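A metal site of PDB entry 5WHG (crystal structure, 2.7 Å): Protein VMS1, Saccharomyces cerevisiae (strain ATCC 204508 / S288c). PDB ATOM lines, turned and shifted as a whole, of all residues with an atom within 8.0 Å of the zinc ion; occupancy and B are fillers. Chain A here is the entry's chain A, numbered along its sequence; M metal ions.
The zinc ion is bound by a ring nitrogen (ND1) of His 68 (1.9 Å). SG of Cys 49 is bound to the zinc ion, at 2.3 Å. The side-chain sulfur (SG) of Cys 46 is bound to the zinc ion, 2.4 Å away. NE2 of His 62 is bound to the zinc ion (2.6 Å). The zinc ion has four donor atoms within binding distance.
OG1 of Thr 65 lies within hydrogen-bond range of N of His 68, 3.3 Å away. A ring nitrogen (ND1) of His 62 sits at hydrogen-bond distance from the side-chain hydroxyl of Thr 65 (2.9 Å). The backbone carbonyl oxygen (O) of Cys 46 is in hydrogen-bond range of the backbone NH (N) of Met 51. N of Val 48 sits close to SG of Cys 46 (3.6 Å). SG of Cys 49 sits close to ND2 of Asn 71, 3.7 Å away.
Residues that only touch the zinc ion: Val 48. Of the 17 residues printed, 5 come within 4 Å of the zinc ion. The nearest printed residue that does not touch the zinc ion is Asn 71 (5.4 Å).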
ATOM      1  N   CYS A  46      14.647 -11.032   0.050  1.00  0.00           N
ATOM      2  CA  CYS A  46      14.409 -11.754   1.303  1.00  0.00           C
ATOM      3  C   CYS A  46      13.228 -12.716   1.213  1.00  0.00           C
ATOM      4  O   CYS A  46      12.087 -12.309   0.968  1.00  0.00           O
ATOM      5  CB  CYS A  46      14.160 -10.796   2.446  1.00  0.00           C
ATOM      6  SG  CYS A  46      13.735 -11.740   3.926  1.00  0.00           S
ATOM      7  N   SER A  47      13.512 -13.999   1.449  1.00  0.00           N
ATOM      8  CA  SER A  47      12.509 -15.030   1.247  1.00  0.00           C
ATOM      9  C   SER A  47      11.599 -15.177   2.453  1.00  0.00           C
ATOM     10  O   SER A  47      10.416 -15.529   2.307  1.00  0.00           O
ATOM     11  CB  SER A  47      13.198 -16.350   0.940  1.00  0.00           C
ATOM     12  OG  SER A  47      14.422 -16.448   1.668  1.00  0.00           O
ATOM     13  N   VAL A  48      12.109 -14.895   3.650  1.00  0.00           N
ATOM     14  CA  VAL A  48      11.317 -15.077   4.863  1.00  0.00           C
ATOM     15  C   VAL A  48      10.395 -13.887   5.137  1.00  0.00           C
ATOM     16  O   VAL A  48       9.456 -14.003   5.925  1.00  0.00           O
ATOM     17  CB  VAL A  48      12.240 -15.350   6.065  1.00  0.00           C
ATOM     18  CG1 VAL A  48      12.912 -14.072   6.516  1.00  0.00           C
ATOM     19  CG2 VAL A  48      11.465 -15.966   7.192  1.00  0.00           C
ATOM     20  N   CYS A  49      10.639 -12.744   4.496  1.00  0.00           N
ATOM     21  CA  CYS A  49       9.777 -11.575   4.611  1.00  0.00           C
ATOM     22  C   CYS A  49       8.894 -11.362   3.399  1.00  0.00           C
ATOM     23  O   CYS A  49       7.986 -10.528   3.477  1.00  0.00           O
ATOM     24  CB  CYS A  49      10.625 -10.317   4.831  1.00  0.00           C
ATOM     25  SG  CYS A  49      11.777 -10.400   6.224  1.00  0.00           S
ATOM     26  N   GLN A  50       9.128 -12.071   2.297  1.00  0.00           N
ATOM     27  CA  GLN A  50       8.451 -11.843   1.022  1.00  0.00           C
ATOM     28  C   GLN A  50       8.618 -10.395   0.562  1.00  0.00           C
ATOM     29  O   GLN A  50       7.690  -9.763   0.059  1.00  0.00           O
ATOM     30  CB  GLN A  50       6.964 -12.228   1.114  1.00  0.00           C
ATOM     31  CG  GLN A  50       6.709 -13.625   1.669  1.00  0.00           C
ATOM     32  CD  GLN A  50       5.224 -13.987   1.743  1.00  0.00           C
ATOM     33  OE1 GLN A  50       4.423 -13.593   0.894  1.00  0.00           O
ATOM     34  NE2 GLN A  50       4.859 -14.756   2.776  1.00  0.00           N
ATOM     35  N   MET A  51       9.838  -9.873   0.728  1.00  0.00           N
ATOM     36  CA  MET A  51      10.125  -8.455   0.541  1.00  0.00           C
ATOM     37  C   MET A  51      11.449  -8.190  -0.210  1.00  0.00           C
ATOM     38  O   MET A  51      12.537  -8.470   0.290  1.00  0.00           O
ATOM     39  CB  MET A  51      10.133  -7.770   1.912  1.00  0.00           C
ATOM     40  CG  MET A  51      10.671  -6.351   1.968  1.00  0.00           C
ATOM     41  SD  MET A  51      10.857  -5.861   3.851  1.00  0.00           S
ATOM     42  CE  MET A  51      12.240  -4.492   3.718  1.00  0.00           C
ATOM     43  N   HIS A  62      18.798  -4.647   4.398  1.00  0.00           N
ATOM     44  CA  HIS A  62      17.741  -5.290   5.175  1.00  0.00           C
ATOM     45  C   HIS A  62      18.178  -6.659   5.650  1.00  0.00           C
ATOM     46  O   HIS A  62      17.696  -7.674   5.178  1.00  0.00           O
ATOM     47  CB  HIS A  62      16.455  -5.392   4.345  1.00  0.00           C
ATOM     48  CG  HIS A  62      15.431  -6.336   4.910  1.00  0.00           C
ATOM     49  ND1 HIS A  62      15.009  -6.296   6.219  1.00  0.00           N
ATOM     50  CD2 HIS A  62      14.775  -7.382   4.342  1.00  0.00           C
ATOM     51  CE1 HIS A  62      14.120  -7.246   6.421  1.00  0.00           C
ATOM     52  NE2 HIS A  62      13.963  -7.929   5.303  1.00  0.00           N
ATOM     53  N   TYR A  63      19.115  -6.708   6.592  1.00  0.00           N
ATOM     54  CA  TYR A  63      19.546  -8.018   7.069  1.00  0.00           C
ATOM     55  C   TYR A  63      20.017  -7.926   8.515  1.00  0.00           C
ATOM     56  O   TYR A  63      20.115  -8.938   9.214  1.00  0.00           O
ATOM     57  CB  TYR A  63      20.645  -8.592   6.169  1.00  0.00           C
ATOM     58  CG  TYR A  63      20.121  -9.639   5.191  1.00  0.00           C
ATOM     59  CD1 TYR A  63      20.023 -10.954   5.567  1.00  0.00           C
ATOM     60  CD2 TYR A  63      19.709  -9.291   3.918  1.00  0.00           C
ATOM     61  CE1 TYR A  63      19.539 -11.909   4.701  1.00  0.00           C
ATOM     62  CE2 TYR A  63      19.210 -10.246   3.036  1.00  0.00           C
ATOM     63  CZ  TYR A  63      19.131 -11.552   3.451  1.00  0.00           C
ATOM     64  OH  TYR A  63      18.645 -12.523   2.592  1.00  0.00           O
ATOM     65  N   GLN A  64      20.324  -6.703   8.944  1.00  0.00           N
ATOM     66  CA  GLN A  64      20.548  -6.402  10.345  1.00  0.00           C
ATOM     67  C   GLN A  64      19.367  -5.668  10.961  1.00  0.00           C
ATOM     68  O   GLN A  64      19.410  -5.344  12.159  1.00  0.00           O
ATOM     69  CB  GLN A  64      21.841  -5.596  10.508  1.00  0.00           C
ATOM     70  CG  GLN A  64      22.886  -6.270  11.383  1.00  0.00           C
ATOM     71  CD  GLN A  64      24.218  -5.539  11.404  1.00  0.00           C
ATOM     72  OE1 GLN A  64      25.168  -5.943  10.734  1.00  0.00           O
ATOM     73  NE2 GLN A  64      24.291  -4.454  12.167  1.00  0.00           N
ATOM     74  N   THR A  65      18.333  -5.392  10.178  1.00  0.00           N
ATOM     75  CA  THR A  65      17.106  -4.804  10.715  1.00  0.00           C
ATOM     76  C   THR A  65      16.468  -5.743  11.734  1.00  0.00           C
ATOM     77  O   THR A  65      16.522  -6.964  11.575  1.00  0.00           O
ATOM     78  CB  THR A  65      16.112  -4.511   9.597  1.00  0.00           C
ATOM     79  OG1 THR A  65      15.647  -5.737   9.041  1.00  0.00           O
ATOM     80  CG2 THR A  65      16.765  -3.691   8.499  1.00  0.00           C
ATOM     81  N   TYR A  67      13.431  -6.151  12.001  1.00  0.00           N
ATOM     82  CA  TYR A  67      12.288  -6.784  11.350  1.00  0.00           C
ATOM     83  C   TYR A  67      12.677  -8.157  10.802  1.00  0.00           C
ATOM     84  O   TYR A  67      12.051  -9.167  11.129  1.00  0.00           O
ATOM     85  CB  TYR A  67      11.756  -5.897  10.232  1.00  0.00           C
ATOM     86  CG  TYR A  67      10.482  -6.407   9.628  1.00  0.00           C
ATOM     87  CD1 TYR A  67       9.312  -6.461  10.359  1.00  0.00           C
ATOM     88  CD2 TYR A  67      10.442  -6.804   8.296  1.00  0.00           C
ATOM     89  CE1 TYR A  67       8.140  -6.919   9.796  1.00  0.00           C
ATOM     90  CE2 TYR A  67       9.276  -7.258   7.727  1.00  0.00           C
ATOM     91  CZ  TYR A  67       8.129  -7.318   8.479  1.00  0.00           C
ATOM     92  OH  TYR A  67       6.964  -7.765   7.898  1.00  0.00           O
ATOM     93  N   HIS A  68      13.712  -8.195   9.948  1.00  0.00           N
ATOM     94  CA  HIS A  68      14.202  -9.462   9.432  1.00  0.00           C
ATOM     95  C   HIS A  68      14.481 -10.472  10.530  1.00  0.00           C
ATOM     96  O   HIS A  68      14.271 -11.675  10.337  1.00  0.00           O
ATOM     97  CB  HIS A  68      15.474  -9.238   8.606  1.00  0.00           C
ATOM     98  CG  HIS A  68      16.047 -10.496   8.031  1.00  0.00           C
ATOM     99  ND1 HIS A  68      15.672 -10.992   6.799  1.00  0.00           N
ATOM    100  CD2 HIS A  68      16.972 -11.361   8.510  1.00  0.00           C
ATOM    101  CE1 HIS A  68      16.334 -12.106   6.549  1.00  0.00           C
ATOM    102  NE2 HIS A  68      17.130 -12.348   7.579  1.00  0.00           N
ATOM    103  N   LEU A  69      14.933 -10.024  11.702  1.00  0.00           N
ATOM    104  CA  LEU A  69      15.307 -10.982  12.726  1.00  0.00           C
ATOM    105  C   LEU A  69      14.083 -11.671  13.333  1.00  0.00           C
ATOM    106  O   LEU A  69      14.115 -12.875  13.604  1.00  0.00           O
ATOM    107  CB  LEU A  69      16.128 -10.289  13.819  1.00  0.00           C
ATOM    108  CG  LEU A  69      17.640 -10.428  13.612  1.00  0.00           C
ATOM    109  CD1 LEU A  69      18.391  -9.808  14.767  1.00  0.00           C
ATOM    110  CD2 LEU A  69      18.010 -11.901  13.432  1.00  0.00           C
ATOM    111  N   MET A  70      13.007 -10.925  13.546  1.00  0.00           N
ATOM    112  CA  MET A  70      11.815 -11.525  14.132  1.00  0.00           C
ATOM    113  C   MET A  70      11.152 -12.485  13.146  1.00  0.00           C
ATOM    114  O   MET A  70      10.626 -13.527  13.538  1.00  0.00           O
ATOM    115  CB  MET A  70      10.840 -10.443  14.580  1.00  0.00           C
ATOM    116  CG  MET A  70      11.458  -9.413  15.500  1.00  0.00           C
ATOM    117  SD  MET A  70      10.278  -7.911  15.915  1.00  0.00           S
ATOM    118  CE  MET A  70       9.168  -8.789  17.259  1.00  0.00           C
ATOM    119  N   ASN A  71      11.183 -12.128  11.853  1.00  0.00           N
ATOM    120  CA  ASN A  71      10.622 -13.008  10.842  1.00  0.00           C
ATOM    121  C   ASN A  71      11.432 -14.293  10.699  1.00  0.00           C
ATOM    122  O   ASN A  71      10.865 -15.377  10.505  1.00  0.00           O
ATOM    123  CB  ASN A  71      10.528 -12.283   9.519  1.00  0.00           C
ATOM    124  CG  ASN A  71       9.244 -11.540   9.382  1.00  0.00           C
ATOM    125  OD1 ASN A  71       8.192 -12.078   9.669  1.00  0.00           O
ATOM    126  ND2 ASN A  71       9.322 -10.296   8.955  1.00  0.00           N
ATOM    127  N   VAL A  72      12.764 -14.189  10.766  1.00  0.00           N
ATOM    128  CA  VAL A  72      13.602 -15.382  10.875  1.00  0.00           C
ATOM    129  C   VAL A  72      13.178 -16.192  12.090  1.00  0.00           C
ATOM    130  O   VAL A  72      12.930 -17.406  12.004  1.00  0.00           O
ATOM    131  CB  VAL A  72      15.090 -15.013  10.946  1.00  0.00           C
ATOM    132  CG1 VAL A  72      15.886 -16.175  11.485  1.00  0.00           C
ATOM    133  CG2 VAL A  72      15.629 -14.622   9.591  1.00  0.00           C
ATOM    134  N   PRO A 204      19.439 -17.738   4.791  1.00  0.00           N
ATOM    135  CA  PRO A 204      19.321 -16.714   5.827  1.00  0.00           C
ATOM    136  C   PRO A 204      18.896 -17.265   7.180  1.00  0.00           C
ATOM    137  O   PRO A 204      19.023 -16.546   8.186  1.00  0.00           O
ATOM    138  CB  PRO A 204      18.261 -15.750   5.257  1.00  0.00           C
ATOM    139  CG  PRO A 204      17.680 -16.455   4.021  1.00  0.00           C
ATOM    140  CD  PRO A 204      18.198 -17.850   4.005  1.00  0.00           C
HETATM  141 ZN    ZN M   1      14.090 -10.444   5.931  1.00  0.00          ZN
